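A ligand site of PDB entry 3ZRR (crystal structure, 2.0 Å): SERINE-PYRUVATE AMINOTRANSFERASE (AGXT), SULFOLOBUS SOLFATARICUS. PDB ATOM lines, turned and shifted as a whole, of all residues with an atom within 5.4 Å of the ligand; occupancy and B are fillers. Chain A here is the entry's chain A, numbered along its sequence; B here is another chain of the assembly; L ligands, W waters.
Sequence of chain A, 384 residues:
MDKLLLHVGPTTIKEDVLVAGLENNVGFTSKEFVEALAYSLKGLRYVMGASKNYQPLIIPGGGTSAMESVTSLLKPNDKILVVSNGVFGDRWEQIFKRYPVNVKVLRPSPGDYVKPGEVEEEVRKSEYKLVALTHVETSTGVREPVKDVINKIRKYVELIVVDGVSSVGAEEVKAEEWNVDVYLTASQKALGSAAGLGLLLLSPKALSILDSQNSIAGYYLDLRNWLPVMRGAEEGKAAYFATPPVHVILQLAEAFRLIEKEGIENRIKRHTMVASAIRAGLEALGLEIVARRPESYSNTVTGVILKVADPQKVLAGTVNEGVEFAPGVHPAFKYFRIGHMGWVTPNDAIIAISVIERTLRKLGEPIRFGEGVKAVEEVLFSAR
The side-chain hydroxyl of Thr 64 sits at hydrogen-bond distance from the guanidinium group of Arg 91 (2.9 Å).
OG1 of Thr 138 is in hydrogen-bond range of OG of Ser 166 (2.6 Å).
The side-chain carboxylate (OD1) of Asp 163 is in hydrogen-bond range of the backbone NH (N) of Val 165, at 2.9 Å.
The side-chain amide nitrogen (NE2) of Gln 188 is in hydrogen-bond range of the side-chain hydroxyl (OG1) of Thr 243 of chain B (3.4 Å).
The backbone NH of Arg 337 sits at hydrogen-bond distance from the backbone carbonyl oxygen of Ala 326 (2.8 Å).
The guanidinium group of Arg 337 lies within hydrogen-bond range of the backbone carbonyl oxygen of Pro 327 (2.8 Å).
N of Phe 88 sits at hydrogen-bond distance from OE2 of Glu 137, at 3.1 Å.
OG of Ser 65 is in hydrogen-bond range of N of Gly 62 (3.0 Å).
Water W1 bridges O7 of the ligand (2.6 Å) and NH1 of Arg 337 (3.5 Å).
Water W3 lies within hydrogen-bond range of O6 of the ligand and NH2 of Arg 337.
Water W2 lies within hydrogen-bond range of the side-chain hydroxyl of Tyr 220 of chain B (2.6 Å), the backbone carbonyl oxygen of Thr 243 of chain B (2.9 Å), an oxygen (O5) of the ligand (2.9 Å) and the backbone NH of Gly 62 (3.4 Å).
The backbone NH (N) of Thr 64 lies within hydrogen-bond range of an oxygen (O5) of the ligand (2.6 Å).
The side-chain hydroxyl of Thr 64 sits at hydrogen-bond distance from an oxygen (O5) of the ligand (2.5 Å).
The side-chain hydroxyl (OG1) of Thr 138 is in hydrogen-bond range of an oxygen (O1) of the ligand, at 2.5 Å.
The side-chain carboxylate of Asp 163 sits at hydrogen-bond distance from a nitrogen (N1) of the ligand, 2.6 Å away.
N of Thr 243 of chain B is in hydrogen-bond range of O4 of the ligand (2.8 Å).
OG1 of Thr 243 of chain B sits at hydrogen-bond distance from O4 of the ligand, at 2.7 Å.
An oxygen (O4) of the ligand sits at hydrogen-bond distance from the side-chain hydroxyl of Tyr 240 of chain B (2.8 Å).
An oxygen (O3) of the ligand sits at hydrogen-bond distance from the backbone NH of Gly 63, 2.9 Å away.
NH2 of Arg 337 lies within salt-bridge range of O7 of the ligand (2.9 Å).
An oxygen (O3) of the ligand sits at hydrogen-bond distance from the side-chain amide nitrogen of Gln 188.
An oxygen (O1) of the ligand is in hydrogen-bond range of the side-chain hydroxyl (OG) of Ser 166 (3.4 Å).
Residues that only touch the ligand: Phe 28 of chain B, Phe 88, Val 165, Gly 62, Val 136, Val 8, Ala 242 of chain B, Met 67, Ala 186 and Lys 189.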
ATOM      1  N   VAL A   8     -13.775  -8.847  25.703  1.00  0.00           N
ATOM      2  CA  VAL A   8     -13.246  -7.953  24.661  1.00  0.00           C
ATOM      3  C   VAL A   8     -12.089  -7.149  25.273  1.00  0.00           C
ATOM      4  O   VAL A   8     -12.242  -6.552  26.337  1.00  0.00           O
ATOM      5  CB  VAL A   8     -14.368  -7.018  24.082  1.00  0.00           C
ATOM      6  CG1 VAL A   8     -13.771  -5.864  23.255  1.00  0.00           C
ATOM      7  CG2 VAL A   8     -15.393  -7.813  23.263  1.00  0.00           C
ATOM      8  N   GLY A  61     -22.050   9.750  24.819  1.00  0.00           N
ATOM      9  CA  GLY A  61     -22.339   8.411  24.357  1.00  0.00           C
ATOM     10  C   GLY A  61     -21.133   7.718  23.781  1.00  0.00           C
ATOM     11  O   GLY A  61     -20.196   7.365  24.513  1.00  0.00           O
ATOM     12  N   GLY A  62     -21.131   7.533  22.466  1.00  0.00           N
ATOM     13  CA  GLY A  62     -19.997   6.865  21.803  1.00  0.00           C
ATOM     14  C   GLY A  62     -20.193   6.857  20.306  1.00  0.00           C
ATOM     15  O   GLY A  62     -20.942   7.698  19.780  1.00  0.00           O
ATOM     16  N   GLY A  63     -19.564   5.908  19.631  1.00  0.00           N
ATOM     17  CA  GLY A  63     -19.752   5.770  18.179  1.00  0.00           C
ATOM     18  C   GLY A  63     -21.235   5.609  17.816  1.00  0.00           C
ATOM     19  O   GLY A  63     -21.688   6.169  16.839  1.00  0.00           O
ATOM     20  N   THR A  64     -21.974   4.865  18.631  1.00  0.00           N
ATOM     21  CA  THR A  64     -23.382   4.582  18.317  1.00  0.00           C
ATOM     22  C   THR A  64     -24.292   5.836  18.402  1.00  0.00           C
ATOM     23  O   THR A  64     -25.151   6.043  17.543  1.00  0.00           O
ATOM     24  CB  THR A  64     -23.948   3.471  19.205  1.00  0.00           C
ATOM     25  OG1 THR A  64     -23.131   2.312  19.077  1.00  0.00           O
ATOM     26  CG2 THR A  64     -25.391   3.122  18.796  1.00  0.00           C
ATOM     27  N   SER A  65     -24.085   6.648  19.417  1.00  0.00           N
ATOM     28  CA  SER A  65     -24.881   7.874  19.558  1.00  0.00           C
ATOM     29  C   SER A  65     -24.489   8.814  18.414  1.00  0.00           C
ATOM     30  O   SER A  65     -25.383   9.436  17.820  1.00  0.00           O
ATOM     31  CB  SER A  65     -24.706   8.525  20.950  1.00  0.00           C
ATOM     32  OG  SER A  65     -23.376   9.004  21.153  1.00  0.00           O
ATOM     33  N   MET A  67     -23.354   7.920  15.369  1.00  0.00           N
ATOM     34  CA  MET A  67     -24.057   7.363  14.201  1.00  0.00           C
ATOM     35  C   MET A  67     -25.554   7.779  14.209  1.00  0.00           C
ATOM     36  O   MET A  67     -26.051   8.313  13.220  1.00  0.00           O
ATOM     37  CB  MET A  67     -23.908   5.829  14.149  1.00  0.00           C
ATOM     38  CG  MET A  67     -22.484   5.328  13.870  1.00  0.00           C
ATOM     39  SD  MET A  67     -22.373   3.580  14.265  1.00  0.00           S
ATOM     40  CE  MET A  67     -23.033   2.830  12.739  1.00  0.00           C
ATOM     41  N   PHE A  88     -20.573  -3.590  12.282  1.00  0.00           N
ATOM     42  CA  PHE A  88     -20.751  -2.163  12.496  1.00  0.00           C
ATOM     43  C   PHE A  88     -21.336  -1.414  11.286  1.00  0.00           C
ATOM     44  O   PHE A  88     -22.041  -0.438  11.441  1.00  0.00           O
ATOM     45  CB  PHE A  88     -19.488  -1.564  13.138  1.00  0.00           C
ATOM     46  CG  PHE A  88     -19.303  -2.028  14.552  1.00  0.00           C
ATOM     47  CD1 PHE A  88     -20.115  -1.527  15.568  1.00  0.00           C
ATOM     48  CD2 PHE A  88     -18.378  -3.031  14.852  1.00  0.00           C
ATOM     49  CE1 PHE A  88     -19.996  -2.002  16.887  1.00  0.00           C
ATOM     50  CE2 PHE A  88     -18.261  -3.526  16.162  1.00  0.00           C
ATOM     51  CZ  PHE A  88     -19.055  -2.992  17.179  1.00  0.00           C
ATOM     52  N   ARG A  91     -24.992  -2.087  11.846  1.00  0.00           N
ATOM     53  CA  ARG A  91     -25.569  -1.215  12.870  1.00  0.00           C
ATOM     54  C   ARG A  91     -26.208   0.050  12.247  1.00  0.00           C
ATOM     55  O   ARG A  91     -27.185   0.555  12.796  1.00  0.00           O
ATOM     56  CB  ARG A  91     -24.520  -0.856  13.949  1.00  0.00           C
ATOM     57  CG  ARG A  91     -25.020   0.144  14.960  1.00  0.00           C
ATOM     58  CD  ARG A  91     -24.317   0.043  16.254  1.00  0.00           C
ATOM     59  NE  ARG A  91     -24.579  -1.228  16.896  1.00  0.00           N
ATOM     60  CZ  ARG A  91     -24.307  -1.476  18.172  1.00  0.00           C
ATOM     61  NH1 ARG A  91     -23.769  -0.517  18.940  1.00  0.00           N
ATOM     62  NH2 ARG A  91     -24.573  -2.666  18.667  1.00  0.00           N
ATOM     63  N   THR A 134     -18.146   2.400   6.440  1.00  0.00           N
ATOM     64  CA  THR A 134     -17.382   2.073   7.633  1.00  0.00           C
ATOM     65  C   THR A 134     -15.900   2.053   7.227  1.00  0.00           C
ATOM     66  O   THR A 134     -15.498   1.212   6.436  1.00  0.00           O
ATOM     67  CB  THR A 134     -17.729   0.691   8.141  1.00  0.00           C
ATOM     68  OG1 THR A 134     -19.165   0.568   8.240  1.00  0.00           O
ATOM     69  CG2 THR A 134     -17.090   0.475   9.507  1.00  0.00           C
ATOM     70  N   VAL A 136     -13.033   1.356   8.990  1.00  0.00           N
ATOM     71  CA  VAL A 136     -12.525   0.038   9.399  1.00  0.00           C
ATOM     72  C   VAL A 136     -13.646  -0.735  10.081  1.00  0.00           C
ATOM     73  O   VAL A 136     -14.249  -0.249  11.053  1.00  0.00           O
ATOM     74  CB  VAL A 136     -11.326   0.136  10.354  1.00  0.00           C
ATOM     75  CG1 VAL A 136     -11.003  -1.247  11.021  1.00  0.00           C
ATOM     76  CG2 VAL A 136     -10.099   0.668   9.618  1.00  0.00           C
ATOM     77  N   GLU A 137     -13.932  -1.920   9.558  1.00  0.00           N
ATOM     78  CA  GLU A 137     -14.957  -2.807  10.114  1.00  0.00           C
ATOM     79  C   GLU A 137     -14.313  -3.655  11.193  1.00  0.00           C
ATOM     80  O   GLU A 137     -13.558  -4.593  10.923  1.00  0.00           O
ATOM     81  CB  GLU A 137     -15.616  -3.691   9.040  1.00  0.00           C
ATOM     82  CG  GLU A 137     -16.544  -4.750   9.611  1.00  0.00           C
ATOM     83  CD  GLU A 137     -17.636  -4.146  10.505  1.00  0.00           C
ATOM     84  OE1 GLU A 137     -18.412  -3.314  10.020  1.00  0.00           O
ATOM     85  OE2 GLU A 137     -17.714  -4.532  11.703  1.00  0.00           O
ATOM     86  N   THR A 138     -14.648  -3.298  12.424  1.00  0.00           N
ATOM     87  CA  THR A 138     -13.977  -3.818  13.602  1.00  0.00           C
ATOM     88  C   THR A 138     -14.183  -5.319  13.737  1.00  0.00           C
ATOM     89  O   THR A 138     -13.288  -6.005  14.227  1.00  0.00           O
ATOM     90  CB  THR A 138     -14.511  -3.077  14.874  1.00  0.00           C
ATOM     91  OG1 THR A 138     -14.413  -1.674  14.645  1.00  0.00           O
ATOM     92  CG2 THR A 138     -13.687  -3.431  16.125  1.00  0.00           C
ATOM     93  N   ASP A 163     -18.204   6.136   9.231  1.00  0.00           N
ATOM     94  CA  ASP A 163     -17.900   5.655  10.575  1.00  0.00           C
ATOM     95  C   ASP A 163     -16.382   5.363  10.677  1.00  0.00           C
ATOM     96  O   ASP A 163     -15.893   4.370  10.119  1.00  0.00           O
ATOM     97  CB  ASP A 163     -18.751   4.413  10.879  1.00  0.00           C
ATOM     98  CG  ASP A 163     -18.323   3.676  12.143  1.00  0.00           C
ATOM     99  OD1 ASP A 163     -17.412   4.138  12.889  1.00  0.00           O
ATOM    100  OD2 ASP A 163     -18.930   2.594  12.356  1.00  0.00           O
ATOM    101  N   VAL A 165     -14.802   5.094  13.761  1.00  0.00           N
ATOM    102  CA  VAL A 165     -14.542   4.679  15.147  1.00  0.00           C
ATOM    103  C   VAL A 165     -13.204   3.904  15.291  1.00  0.00           C
ATOM    104  O   VAL A 165     -12.404   4.210  16.186  1.00  0.00           O
ATOM    105  CB  VAL A 165     -15.711   3.886  15.770  1.00  0.00           C
ATOM    106  CG1 VAL A 165     -15.298   3.223  17.088  1.00  0.00           C
ATOM    107  CG2 VAL A 165     -16.937   4.802  16.001  1.00  0.00           C
ATOM    108  N   SER A 166     -12.930   2.966  14.373  1.00  0.00           N
ATOM    109  CA  SER A 166     -11.682   2.194  14.406  1.00  0.00           C
ATOM    110  C   SER A 166     -10.633   2.679  13.415  1.00  0.00           C
ATOM    111  O   SER A 166      -9.745   1.896  13.027  1.00  0.00           O
ATOM    112  CB  SER A 166     -11.945   0.706  14.140  1.00  0.00           C
ATOM    113  OG  SER A 166     -12.636   0.108  15.183  1.00  0.00           O
ATOM    114  N   ALA A 186     -15.336   7.797  18.111  1.00  0.00           N
ATOM    115  CA  ALA A 186     -15.658   7.726  19.516  1.00  0.00           C
ATOM    116  C   ALA A 186     -14.397   8.071  20.303  1.00  0.00           C
ATOM    117  O   ALA A 186     -13.317   8.168  19.731  1.00  0.00           O
ATOM    118  CB  ALA A 186     -16.195   6.334  19.882  1.00  0.00           C
ATOM    119  N   GLN A 188     -12.954   6.279  22.778  1.00  0.00           N
ATOM    120  CA  GLN A 188     -12.242   5.176  23.451  1.00  0.00           C
ATOM    121  C   GLN A 188     -11.470   4.231  22.534  1.00  0.00           C
ATOM    122  O   GLN A 188     -10.912   3.256  23.022  1.00  0.00           O
ATOM    123  CB  GLN A 188     -13.191   4.354  24.346  1.00  0.00           C
ATOM    124  CG  GLN A 188     -14.109   3.313  23.646  1.00  0.00           C
ATOM    125  CD  GLN A 188     -15.292   3.956  22.905  1.00  0.00           C
ATOM    126  OE1 GLN A 188     -15.529   5.159  22.993  1.00  0.00           O
ATOM    127  NE2 GLN A 188     -16.032   3.138  22.155  1.00  0.00           N
ATOM    128  N   LYS A 189     -11.422   4.495  21.223  1.00  0.00           N
ATOM    129  CA  LYS A 189     -10.774   3.524  20.332  1.00  0.00           C
ATOM    130  C   LYS A 189      -9.389   4.021  19.889  1.00  0.00           C
ATOM    131  O   LYS A 189      -8.501   4.204  20.732  1.00  0.00           O
ATOM    132  CB  LYS A 189     -11.710   3.107  19.177  1.00  0.00           C
ATOM    133  CG  LYS A 189     -12.882   2.211  19.623  1.00  0.00           C
ATOM    134  CD  LYS A 189     -12.392   0.845  20.082  1.00  0.00           C
ATOM    135  CE  LYS A 189     -13.386   0.092  20.965  1.00  0.00           C
ATOM    136  NZ  LYS A 189     -12.825  -1.268  21.353  1.00  0.00           N
ATOM    137  N   ALA A 326      -9.905 -10.065  21.401  1.00  0.00           N
ATOM    138  CA  ALA A 326     -11.355 -10.026  21.403  1.00  0.00           C
ATOM    139  C   ALA A 326     -11.897 -11.164  20.535  1.00  0.00           C
ATOM    140  O   ALA A 326     -11.172 -11.689  19.681  1.00  0.00           O
ATOM    141  CB  ALA A 326     -11.838  -8.650  20.871  1.00  0.00           C
ATOM    142  N   PRO A 327     -13.186 -11.545  20.729  1.00  0.00           N
ATOM    143  CA  PRO A 327     -13.730 -12.681  19.989  1.00  0.00           C
ATOM    144  C   PRO A 327     -13.981 -12.336  18.532  1.00  0.00           C
ATOM    145  O   PRO A 327     -14.114 -11.156  18.172  1.00  0.00           O
ATOM    146  CB  PRO A 327     -15.075 -12.962  20.695  1.00  0.00           C
ATOM    147  CG  PRO A 327     -15.073 -12.138  21.952  1.00  0.00           C
ATOM    148  CD  PRO A 327     -14.209 -10.944  21.611  1.00  0.00           C
ATOM    149  N   ARG A 337      -9.573 -11.842  17.440  1.00  0.00           N
ATOM    150  CA  ARG A 337      -9.069 -10.607  16.858  1.00  0.00           C
ATOM    151  C   ARG A 337      -8.024  -9.974  17.762  1.00  0.00           C
ATOM    152  O   ARG A 337      -8.083 -10.105  18.975  1.00  0.00           O
ATOM    153  CB  ARG A 337     -10.222  -9.620  16.637  1.00  0.00           C
ATOM    154  CG  ARG A 337     -11.114 -10.011  15.493  1.00  0.00           C
ATOM    155  CD  ARG A 337     -12.287  -9.029  15.325  1.00  0.00           C
ATOM    156  NE  ARG A 337     -13.164  -9.112  16.485  1.00  0.00           N
ATOM    157  CZ  ARG A 337     -13.452  -8.095  17.283  1.00  0.00           C
ATOM    158  NH1 ARG A 337     -12.946  -6.896  17.032  1.00  0.00           N
ATOM    159  NH2 ARG A 337     -14.246  -8.297  18.320  1.00  0.00           N
ATOM    160  N   PHE B  28     -15.570  -2.656  29.063  1.00  0.00           N
ATOM    161  CA  PHE B  28     -16.913  -3.102  29.421  1.00  0.00           C
ATOM    162  C   PHE B  28     -17.032  -4.620  29.754  1.00  0.00           C
ATOM    163  O   PHE B  28     -18.045  -5.041  30.332  1.00  0.00           O
ATOM    164  CB  PHE B  28     -17.930  -2.672  28.360  1.00  0.00           C
ATOM    165  CG  PHE B  28     -17.834  -3.444  27.077  1.00  0.00           C
ATOM    166  CD1 PHE B  28     -16.956  -3.058  26.072  1.00  0.00           C
ATOM    167  CD2 PHE B  28     -18.651  -4.548  26.866  1.00  0.00           C
ATOM    168  CE1 PHE B  28     -16.879  -3.762  24.886  1.00  0.00           C
ATOM    169  CE2 PHE B  28     -18.576  -5.272  25.671  1.00  0.00           C
ATOM    170  CZ  PHE B  28     -17.686  -4.874  24.671  1.00  0.00           C
ATOM    171  N   TYR B 220     -30.512   4.365  20.393  1.00  0.00           N
ATOM    172  CA  TYR B 220     -29.627   4.541  21.569  1.00  0.00           C
ATOM    173  C   TYR B 220     -30.385   4.667  22.892  1.00  0.00           C
ATOM    174  O   TYR B 220     -29.910   4.172  23.936  1.00  0.00           O
ATOM    175  CB  TYR B 220     -28.773   5.780  21.373  1.00  0.00           C
ATOM    176  CG  TYR B 220     -27.443   5.731  22.145  1.00  0.00           C
ATOM    177  CD1 TYR B 220     -26.441   4.795  21.826  1.00  0.00           C
ATOM    178  CD2 TYR B 220     -27.177   6.667  23.133  1.00  0.00           C
ATOM    179  CE1 TYR B 220     -25.236   4.787  22.516  1.00  0.00           C
ATOM    180  CE2 TYR B 220     -25.931   6.669  23.809  1.00  0.00           C
ATOM    181  CZ  TYR B 220     -24.979   5.735  23.479  1.00  0.00           C
ATOM    182  OH  TYR B 220     -23.767   5.722  24.148  1.00  0.00           O
ATOM    183  N   TYR B 240     -22.853  -6.633  25.446  1.00  0.00           N
ATOM    184  CA  TYR B 240     -22.573  -5.440  24.676  1.00  0.00           C
ATOM    185  C   TYR B 240     -23.812  -4.951  23.961  1.00  0.00           C
ATOM    186  O   TYR B 240     -24.396  -5.684  23.195  1.00  0.00           O
ATOM    187  CB  TYR B 240     -21.488  -5.730  23.639  1.00  0.00           C
ATOM    188  CG  TYR B 240     -21.251  -4.540  22.746  1.00  0.00           C
ATOM    189  CD1 TYR B 240     -20.715  -3.362  23.265  1.00  0.00           C
ATOM    190  CD2 TYR B 240     -21.615  -4.570  21.395  1.00  0.00           C
ATOM    191  CE1 TYR B 240     -20.504  -2.228  22.440  1.00  0.00           C
ATOM    192  CE2 TYR B 240     -21.415  -3.448  20.565  1.00  0.00           C
ATOM    193  CZ  TYR B 240     -20.854  -2.290  21.092  1.00  0.00           C
ATOM    194  OH  TYR B 240     -20.664  -1.176  20.281  1.00  0.00           O
ATOM    195  N   ALA B 242     -23.905  -0.920  23.420  1.00  0.00           N
ATOM    196  CA  ALA B 242     -23.051   0.209  22.948  1.00  0.00           C
ATOM    197  C   ALA B 242     -22.087   0.506  24.103  1.00  0.00           C
ATOM    198  O   ALA B 242     -22.409   0.209  25.276  1.00  0.00           O
ATOM    199  CB  ALA B 242     -23.876   1.440  22.607  1.00  0.00           C
ATOM    200  N   THR B 243     -20.911   1.044  23.811  1.00  0.00           N
ATOM    201  CA  THR B 243     -19.909   1.204  24.863  1.00  0.00           C
ATOM    202  C   THR B 243     -20.413   2.223  25.896  1.00  0.00           C
ATOM    203  O   THR B 243     -20.758   3.348  25.518  1.00  0.00           O
ATOM    204  CB  THR B 243     -18.524   1.664  24.279  1.00  0.00           C
ATOM    205  OG1 THR B 243     -18.054   0.678  23.357  1.00  0.00           O
ATOM    206  CG2 THR B 243     -17.469   1.830  25.428  1.00  0.00           C
HETATM  207  N1  LIG L   1     -18.502   1.611  14.716  1.00  0.00           N
HETATM  208  C1  LIG L   1     -17.378   0.881  14.850  1.00  0.00           C
HETATM  209  C2  LIG L   1     -16.482   0.641  13.646  1.00  0.00           C
HETATM  210  C3  LIG L   1     -17.026   0.382  16.112  1.00  0.00           C
HETATM  211  O1  LIG L   1     -15.877  -0.325  16.219  1.00  0.00           O
HETATM  212  C4  LIG L   1     -18.998   1.349  17.049  1.00  0.00           C
HETATM  213  C5  LIG L   1     -19.318   1.860  15.769  1.00  0.00           C
HETATM  214  C6  LIG L   1     -19.931   1.635  18.235  1.00  0.00           C
HETATM  215  O2  LIG L   1     -19.233   2.461  19.166  1.00  0.00           O
HETATM  216  P1  LIG L   1     -19.758   2.631  20.651  1.00  0.00           P
HETATM  217  O3  LIG L   1     -18.796   3.642  21.213  1.00  0.00           O
HETATM  218  O4  LIG L   1     -19.704   1.233  21.243  1.00  0.00           O
HETATM  219  O5  LIG L   1     -21.179   3.106  20.427  1.00  0.00           O
HETATM  220  C7  LIG L   1     -17.834   0.615  17.220  1.00  0.00           C
HETATM  221  C8  LIG L   1     -17.488   0.105  18.609  1.00  0.00           C
HETATM  222  C9  LIG L   1     -15.643  -5.608  19.922  1.00  0.00           C
HETATM  223  C10 LIG L   1     -16.183  -4.230  20.205  1.00  0.00           C
HETATM  224  O6  LIG L   1     -16.401  -6.595  20.070  1.00  0.00           O
HETATM  225  C11 LIG L   1     -16.051  -3.196  19.265  1.00  0.00           C
HETATM  226  C12 LIG L   1     -16.561  -1.931  19.542  1.00  0.00           C
HETATM  227  C13 LIG L   1     -17.192  -1.720  20.777  1.00  0.00           C
HETATM  228  C14 LIG L   1     -17.320  -2.746  21.711  1.00  0.00           C
HETATM  229  C15 LIG L   1     -16.806  -4.004  21.429  1.00  0.00           C
HETATM  230  O7  LIG L   1     -14.443  -5.695  19.562  1.00  0.00           O
HETATM  231  N2  LIG L   1     -16.451  -0.921  18.645  1.00  0.00           N
HETATM  232  O   HOH W   1     -12.109  -4.554  19.485  1.00  0.00           O
HETATM  233  O   HOH W   2     -21.901   4.280  23.024  1.00  0.00           O
HETATM  234  O   HOH W   3     -16.956  -9.204  19.725  1.00  0.00           O
